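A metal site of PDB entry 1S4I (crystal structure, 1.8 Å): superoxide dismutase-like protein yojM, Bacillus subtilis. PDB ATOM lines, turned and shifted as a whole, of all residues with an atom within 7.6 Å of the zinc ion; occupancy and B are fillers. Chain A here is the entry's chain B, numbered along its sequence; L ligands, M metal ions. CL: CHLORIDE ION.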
ATOM      1  N   PHE A  64      -5.344 -12.333 -17.142  1.00  0.00           N
ATOM      2  CA  PHE A  64      -4.868 -13.737 -17.185  1.00  0.00           C
ATOM      3  C   PHE A  64      -6.153 -14.545 -17.475  1.00  0.00           C
ATOM      4  O   PHE A  64      -7.010 -14.457 -16.694  1.00  0.00           O
ATOM      5  CB  PHE A  64      -4.371 -14.142 -15.808  1.00  0.00           C
ATOM      6  CG  PHE A  64      -3.951 -15.639 -15.614  1.00  0.00           C
ATOM      7  CD1 PHE A  64      -3.182 -16.377 -16.547  1.00  0.00           C
ATOM      8  CD2 PHE A  64      -4.210 -16.223 -14.377  1.00  0.00           C
ATOM      9  CE1 PHE A  64      -2.759 -17.736 -16.222  1.00  0.00           C
ATOM     10  CE2 PHE A  64      -3.799 -17.566 -14.042  1.00  0.00           C
ATOM     11  CZ  PHE A  64      -3.180 -18.315 -14.981  1.00  0.00           C
ATOM     12  N   HIS A  65      -6.213 -15.256 -18.576  1.00  0.00           N
ATOM     13  CA  HIS A  65      -7.435 -15.957 -19.047  1.00  0.00           C
ATOM     14  C   HIS A  65      -7.146 -17.296 -19.650  1.00  0.00           C
ATOM     15  O   HIS A  65      -6.052 -17.630 -20.067  1.00  0.00           O
ATOM     16  CB  HIS A  65      -8.396 -15.121 -19.982  1.00  0.00           C
ATOM     17  CG  HIS A  65      -8.459 -13.647 -19.669  1.00  0.00           C
ATOM     18  ND1 HIS A  65      -8.165 -12.705 -20.609  1.00  0.00           N
ATOM     19  CD2 HIS A  65      -8.701 -12.969 -18.509  1.00  0.00           C
ATOM     20  CE1 HIS A  65      -8.251 -11.493 -20.071  1.00  0.00           C
ATOM     21  NE2 HIS A  65      -8.535 -11.627 -18.791  1.00  0.00           N
ATOM     22  N   ILE A  66      -8.183 -18.117 -19.697  1.00  0.00           N
ATOM     23  CA  ILE A  66      -8.056 -19.443 -20.407  1.00  0.00           C
ATOM     24  C   ILE A  66      -8.754 -19.270 -21.750  1.00  0.00           C
ATOM     25  O   ILE A  66      -9.915 -18.724 -21.853  1.00  0.00           O
ATOM     26  CB  ILE A  66      -8.815 -20.557 -19.563  1.00  0.00           C
ATOM     27  CG1 ILE A  66      -8.237 -20.575 -18.161  1.00  0.00           C
ATOM     28  CG2 ILE A  66      -8.730 -21.916 -20.296  1.00  0.00           C
ATOM     29  CD1 ILE A  66      -8.806 -21.754 -17.235  1.00  0.00           C
ATOM     30  N   TYR A  67      -8.028 -19.665 -22.807  1.00  0.00           N
ATOM     31  CA  TYR A  67      -8.467 -19.495 -24.182  1.00  0.00           C
ATOM     32  C   TYR A  67      -8.739 -20.890 -24.732  1.00  0.00           C
ATOM     33  O   TYR A  67      -8.247 -21.916 -24.158  1.00  0.00           O
ATOM     34  CB  TYR A  67      -7.362 -18.736 -24.990  1.00  0.00           C
ATOM     35  CG  TYR A  67      -7.333 -17.256 -24.570  1.00  0.00           C
ATOM     36  CD1 TYR A  67      -8.136 -16.299 -25.239  1.00  0.00           C
ATOM     37  CD2 TYR A  67      -6.615 -16.840 -23.423  1.00  0.00           C
ATOM     38  CE1 TYR A  67      -8.160 -14.964 -24.855  1.00  0.00           C
ATOM     39  CE2 TYR A  67      -6.647 -15.515 -23.047  1.00  0.00           C
ATOM     40  CZ  TYR A  67      -7.393 -14.580 -23.769  1.00  0.00           C
ATOM     41  OH  TYR A  67      -7.456 -13.290 -23.326  1.00  0.00           O
ATOM     42  N   PRO A  83     -11.585 -16.618 -26.054  1.00  0.00           N
ATOM     43  CA  PRO A  83     -11.934 -17.090 -24.696  1.00  0.00           C
ATOM     44  C   PRO A  83     -12.613 -18.426 -24.522  1.00  0.00           C
ATOM     45  O   PRO A  83     -13.482 -18.807 -25.270  1.00  0.00           O
ATOM     46  CB  PRO A  83     -12.729 -15.909 -24.074  1.00  0.00           C
ATOM     47  CG  PRO A  83     -12.711 -14.798 -25.125  1.00  0.00           C
ATOM     48  CD  PRO A  83     -12.251 -15.351 -26.402  1.00  0.00           C
ATOM     49  N   PHE A  84     -12.181 -19.157 -23.517  1.00  0.00           N
ATOM     50  CA  PHE A  84     -12.907 -20.378 -23.180  1.00  0.00           C
ATOM     51  C   PHE A  84     -14.238 -19.961 -22.617  1.00  0.00           C
ATOM     52  O   PHE A  84     -14.311 -19.344 -21.566  1.00  0.00           O
ATOM     53  CB  PHE A  84     -12.138 -21.215 -22.173  1.00  0.00           C
ATOM     54  CG  PHE A  84     -12.842 -22.464 -21.756  1.00  0.00           C
ATOM     55  CD1 PHE A  84     -13.293 -22.632 -20.460  1.00  0.00           C
ATOM     56  CD2 PHE A  84     -13.029 -23.496 -22.675  1.00  0.00           C
ATOM     57  CE1 PHE A  84     -13.946 -23.903 -20.104  1.00  0.00           C
ATOM     58  CE2 PHE A  84     -13.662 -24.707 -22.303  1.00  0.00           C
ATOM     59  CZ  PHE A  84     -14.121 -24.870 -21.075  1.00  0.00           C
ATOM     60  N   ASN A  85     -15.320 -20.240 -23.356  1.00  0.00           N
ATOM     61  CA  ASN A  85     -16.593 -19.577 -23.068  1.00  0.00           C
ATOM     62  C   ASN A  85     -17.767 -20.510 -23.445  1.00  0.00           C
ATOM     63  O   ASN A  85     -18.587 -20.129 -24.260  1.00  0.00           O
ATOM     64  CB  ASN A  85     -16.698 -18.207 -23.795  1.00  0.00           C
ATOM     65  CG  ASN A  85     -17.955 -17.401 -23.396  1.00  0.00           C
ATOM     66  OD1 ASN A  85     -18.520 -17.624 -22.320  1.00  0.00           O
ATOM     67  ND2 ASN A  85     -18.395 -16.446 -24.291  1.00  0.00           N
ATOM     68  N   LYS A  89     -21.108 -16.252 -22.466  1.00  0.00           N
ATOM     69  CA  LYS A  89     -21.436 -15.069 -21.679  1.00  0.00           C
ATOM     70  C   LYS A  89     -20.589 -13.993 -22.258  1.00  0.00           C
ATOM     71  O   LYS A  89     -19.808 -14.241 -23.170  1.00  0.00           O
ATOM     72  CB  LYS A  89     -21.079 -15.353 -20.220  1.00  0.00           C
ATOM     73  CG  LYS A  89     -21.564 -16.743 -19.856  1.00  0.00           C
ATOM     74  CD  LYS A  89     -21.730 -16.897 -18.367  1.00  0.00           C
ATOM     75  CE  LYS A  89     -22.763 -15.937 -17.805  1.00  0.00           C
ATOM     76  NZ  LYS A  89     -24.158 -16.561 -17.931  1.00  0.00           N
ATOM     77  N   GLU A  90     -20.707 -12.766 -21.770  1.00  0.00           N
ATOM     78  CA  GLU A  90     -19.637 -11.905 -22.216  1.00  0.00           C
ATOM     79  C   GLU A  90     -18.530 -11.823 -21.110  1.00  0.00           C
ATOM     80  O   GLU A  90     -18.657 -12.508 -20.069  1.00  0.00           O
ATOM     81  CB  GLU A  90     -20.100 -10.577 -22.724  1.00  0.00           C
ATOM     82  CG  GLU A  90     -20.765  -9.685 -21.740  1.00  0.00           C
ATOM     83  CD  GLU A  90     -21.725  -8.742 -22.461  1.00  0.00           C
ATOM     84  OE1 GLU A  90     -21.402  -7.548 -22.559  1.00  0.00           O
ATOM     85  OE2 GLU A  90     -22.815  -9.185 -22.915  1.00  0.00           O
ATOM     86  N   HIS A  91     -17.524 -10.982 -21.331  1.00  0.00           N
ATOM     87  CA  HIS A  91     -16.373 -10.811 -20.442  1.00  0.00           C
ATOM     88  C   HIS A  91     -16.601 -10.079 -19.128  1.00  0.00           C
ATOM     89  O   HIS A  91     -17.173  -8.974 -19.104  1.00  0.00           O
ATOM     90  CB  HIS A  91     -15.233 -10.053 -21.165  1.00  0.00           C
ATOM     91  CG  HIS A  91     -13.970  -9.952 -20.335  1.00  0.00           C
ATOM     92  ND1 HIS A  91     -13.086 -11.001 -20.204  1.00  0.00           N
ATOM     93  CD2 HIS A  91     -13.529  -8.980 -19.498  1.00  0.00           C
ATOM     94  CE1 HIS A  91     -12.120 -10.657 -19.355  1.00  0.00           C
ATOM     95  NE2 HIS A  91     -12.352  -9.426 -18.922  1.00  0.00           N
ATOM     96  N   GLY A  92     -16.050 -10.648 -18.058  1.00  0.00           N
ATOM     97  CA  GLY A  92     -15.695  -9.898 -16.889  1.00  0.00           C
ATOM     98  C   GLY A  92     -16.488 -10.132 -15.643  1.00  0.00           C
ATOM     99  O   GLY A  92     -17.745 -10.118 -15.701  1.00  0.00           O
ATOM    100  N   PHE A  93     -15.787 -10.245 -14.505  1.00  0.00           N
ATOM    101  CA  PHE A  93     -16.431 -10.380 -13.208  1.00  0.00           C
ATOM    102  C   PHE A  93     -17.441  -9.221 -12.963  1.00  0.00           C
ATOM    103  O   PHE A  93     -18.503  -9.443 -12.383  1.00  0.00           O
ATOM    104  CB  PHE A  93     -15.429 -10.531 -12.025  1.00  0.00           C
ATOM    105  CG  PHE A  93     -14.443 -11.664 -12.190  1.00  0.00           C
ATOM    106  CD1 PHE A  93     -13.099 -11.433 -12.062  1.00  0.00           C
ATOM    107  CD2 PHE A  93     -14.868 -12.930 -12.538  1.00  0.00           C
ATOM    108  CE1 PHE A  93     -12.175 -12.449 -12.285  1.00  0.00           C
ATOM    109  CE2 PHE A  93     -13.977 -13.967 -12.740  1.00  0.00           C
ATOM    110  CZ  PHE A  93     -12.578 -13.687 -12.597  1.00  0.00           C
ATOM    111  N   HIS A  99     -19.937 -13.495 -17.711  1.00  0.00           N
ATOM    112  CA  HIS A  99     -18.800 -14.087 -17.046  1.00  0.00           C
ATOM    113  C   HIS A  99     -18.169 -15.185 -17.902  1.00  0.00           C
ATOM    114  O   HIS A  99     -18.695 -16.298 -17.876  1.00  0.00           O
ATOM    115  CB  HIS A  99     -19.366 -14.629 -15.740  1.00  0.00           C
ATOM    116  CG  HIS A  99     -18.339 -14.991 -14.701  1.00  0.00           C
ATOM    117  ND1 HIS A  99     -18.361 -14.448 -13.435  1.00  0.00           N
ATOM    118  CD2 HIS A  99     -17.364 -15.936 -14.709  1.00  0.00           C
ATOM    119  CE1 HIS A  99     -17.436 -15.036 -12.710  1.00  0.00           C
ATOM    120  NE2 HIS A  99     -16.842 -15.965 -13.452  1.00  0.00           N
ATOM    121  N   HIS A 100     -17.077 -14.982 -18.662  1.00  0.00           N
ATOM    122  CA  HIS A 100     -16.557 -16.195 -19.329  1.00  0.00           C
ATOM    123  C   HIS A 100     -16.005 -17.167 -18.305  1.00  0.00           C
ATOM    124  O   HIS A 100     -15.413 -16.722 -17.313  1.00  0.00           O
ATOM    125  CB  HIS A 100     -15.434 -15.970 -20.291  1.00  0.00           C
ATOM    126  CG  HIS A 100     -15.720 -14.941 -21.347  1.00  0.00           C
ATOM    127  ND1 HIS A 100     -14.774 -13.972 -21.699  1.00  0.00           N
ATOM    128  CD2 HIS A 100     -16.767 -14.759 -22.181  1.00  0.00           C
ATOM    129  CE1 HIS A 100     -15.252 -13.237 -22.696  1.00  0.00           C
ATOM    130  NE2 HIS A 100     -16.448 -13.710 -23.031  1.00  0.00           N
ATOM    131  N   ALA A 101     -16.145 -18.474 -18.574  1.00  0.00           N
ATOM    132  CA  ALA A 101     -15.650 -19.508 -17.687  1.00  0.00           C
ATOM    133  C   ALA A 101     -14.077 -19.457 -17.561  1.00  0.00           C
ATOM    134  O   ALA A 101     -13.529 -19.899 -16.576  1.00  0.00           O
ATOM    135  CB  ALA A 101     -16.036 -20.872 -18.252  1.00  0.00           C
ATOM    136  N   GLY A 102     -13.459 -18.974 -18.604  1.00  0.00           N
ATOM    137  CA  GLY A 102     -11.976 -18.834 -18.665  1.00  0.00           C
ATOM    138  C   GLY A 102     -11.418 -17.517 -18.088  1.00  0.00           C
ATOM    139  O   GLY A 102     -10.172 -17.273 -18.086  1.00  0.00           O
ATOM    140  N   ASP A 103     -12.283 -16.663 -17.578  1.00  0.00           N
ATOM    141  CA  ASP A 103     -11.878 -15.465 -16.868  1.00  0.00           C
ATOM    142  C   ASP A 103     -11.329 -15.729 -15.491  1.00  0.00           C
ATOM    143  O   ASP A 103     -12.019 -16.286 -14.636  1.00  0.00           O
ATOM    144  CB  ASP A 103     -13.037 -14.444 -16.727  1.00  0.00           C
ATOM    145  CG  ASP A 103     -13.433 -13.848 -18.023  1.00  0.00           C
ATOM    146  OD1 ASP A 103     -14.506 -13.195 -18.057  1.00  0.00           O
ATOM    147  OD2 ASP A 103     -12.742 -13.972 -19.070  1.00  0.00           O
ATOM    148  N   LEU A 104     -10.078 -15.301 -15.234  1.00  0.00           N
ATOM    149  CA  LEU A 104      -9.403 -15.469 -13.997  1.00  0.00           C
ATOM    150  C   LEU A 104      -8.965 -14.089 -13.441  1.00  0.00           C
ATOM    151  O   LEU A 104      -8.858 -13.151 -14.228  1.00  0.00           O
ATOM    152  CB  LEU A 104      -8.149 -16.367 -14.194  1.00  0.00           C
ATOM    153  CG  LEU A 104      -8.298 -17.771 -14.891  1.00  0.00           C
ATOM    154  CD1 LEU A 104      -6.990 -18.608 -14.973  1.00  0.00           C
ATOM    155  CD2 LEU A 104      -9.417 -18.704 -14.282  1.00  0.00           C
ATOM    156  N   ASP A 149      -6.691  -6.475 -16.552  1.00  0.00           N
ATOM    157  CA  ASP A 149      -8.004  -6.717 -17.079  1.00  0.00           C
ATOM    158  C   ASP A 149      -8.871  -5.807 -16.260  1.00  0.00           C
ATOM    159  O   ASP A 149      -8.655  -5.683 -15.059  1.00  0.00           O
ATOM    160  CB  ASP A 149      -8.282  -8.227 -16.795  1.00  0.00           C
ATOM    161  CG  ASP A 149      -9.676  -8.713 -17.274  1.00  0.00           C
ATOM    162  OD1 ASP A 149     -10.653  -7.913 -17.447  1.00  0.00           O
ATOM    163  OD2 ASP A 149      -9.844  -9.950 -17.457  1.00  0.00           O
ATOM    164  N   THR A 153     -14.857  -4.693 -19.929  1.00  0.00           N
ATOM    165  CA  THR A 153     -14.891  -4.523 -21.401  1.00  0.00           C
ATOM    166  C   THR A 153     -14.755  -5.846 -22.153  1.00  0.00           C
ATOM    167  O   THR A 153     -13.958  -6.710 -21.789  1.00  0.00           O
ATOM    168  CB  THR A 153     -13.700  -3.630 -21.819  1.00  0.00           C
ATOM    169  OG1 THR A 153     -13.733  -2.445 -21.015  1.00  0.00           O
ATOM    170  CG2 THR A 153     -13.806  -3.146 -23.190  1.00  0.00           C
ATOM    171  N   ASN A 154     -15.525  -5.978 -23.228  1.00  0.00           N
ATOM    172  CA  ASN A 154     -15.385  -7.129 -24.115  1.00  0.00           C
ATOM    173  C   ASN A 154     -14.330  -6.942 -25.204  1.00  0.00           C
ATOM    174  O   ASN A 154     -14.138  -5.804 -25.582  1.00  0.00           O
ATOM    175  CB  ASN A 154     -16.712  -7.305 -24.834  1.00  0.00           C
ATOM    176  CG  ASN A 154     -17.653  -7.993 -24.012  1.00  0.00           C
ATOM    177  OD1 ASN A 154     -17.380  -9.134 -23.613  1.00  0.00           O
ATOM    178  ND2 ASN A 154     -18.785  -7.323 -23.674  1.00  0.00           N
ATOM    179  N   PRO A 155     -13.709  -8.005 -25.770  1.00  0.00           N
ATOM    180  CA  PRO A 155     -13.805  -9.412 -25.321  1.00  0.00           C
ATOM    181  C   PRO A 155     -12.952  -9.844 -24.132  1.00  0.00           C
ATOM    182  O   PRO A 155     -13.201 -10.902 -23.464  1.00  0.00           O
ATOM    183  CB  PRO A 155     -13.351 -10.233 -26.579  1.00  0.00           C
ATOM    184  CG  PRO A 155     -12.426  -9.316 -27.360  1.00  0.00           C
ATOM    185  CD  PRO A 155     -12.884  -7.873 -27.009  1.00  0.00           C
ATOM    186  N   SER A 156     -11.933  -9.047 -23.866  1.00  0.00           N
ATOM    187  CA  SER A 156     -10.912  -9.438 -22.911  1.00  0.00           C
ATOM    188  C   SER A 156     -10.513  -8.398 -21.845  1.00  0.00           C
ATOM    189  O   SER A 156      -9.403  -8.501 -21.267  1.00  0.00           O
ATOM    190  CB  SER A 156      -9.653  -9.838 -23.690  1.00  0.00           C
ATOM    191  OG  SER A 156      -8.738  -8.757 -23.586  1.00  0.00           O
ATOM    192  N   GLY A 157     -11.400  -7.447 -21.556  1.00  0.00           N
ATOM    193  CA  GLY A 157     -11.207  -6.629 -20.379  1.00  0.00           C
ATOM    194  C   GLY A 157     -10.187  -5.523 -20.624  1.00  0.00           C
ATOM    195  O   GLY A 157      -9.660  -4.909 -19.682  1.00  0.00           O
HETATM  196 CL    CL L   1     -11.214 -13.299 -21.747  1.00  0.00          CL
HETATM  197 ZN    ZN M   1     -13.035 -13.117 -20.781  1.00  0.00          ZN
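The side-chain carboxylate (OD1) of Asp 103 sits at hydrogen-bond distance from the backbone NH (N) of Gly 92 (3.0 Å).
N of His 100 lies within hydrogen-bond range of O of Glu 90, 3.3 Å away.
NE2 of His 100 sits close to O of Lys 89, 3.4 Å away.
A ring nitrogen (ND1) of His 91 lies close to the backbone carbonyl oxygen (O) of Pro 155 (3.3 Å).
OD1 of Asp 149 is in hydrogen-bond range of NE2 of His 91 (2.7 Å).
A ring nitrogen (NE2) of His 91 lies close to the backbone NH (N) of Gly 157 (3.4 Å).
The side-chain amide oxygen (OD1) of Asn 154 is in hydrogen-bond range of the backbone NH (N) of His 91 (2.9 Å).
Residues that only touch the zinc ion: Pro 155 (3.5 Å).
Four residues have an atom within 4 Å of the zinc ion: His 91, His 100, Asp 103 and Pro 155.
The zinc ion is bound by OD2 of Asp 103 (1.9 Å).
A chlorine (CL) of the ligand binds the zinc ion, 2.1 Å away.
ND1 of His 100 binds the zinc ion, 2.1 Å away.
The zinc ion is bound by ND1 of His 91, 2.2 Å away.
The zinc ion has four donor atoms within binding distance.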
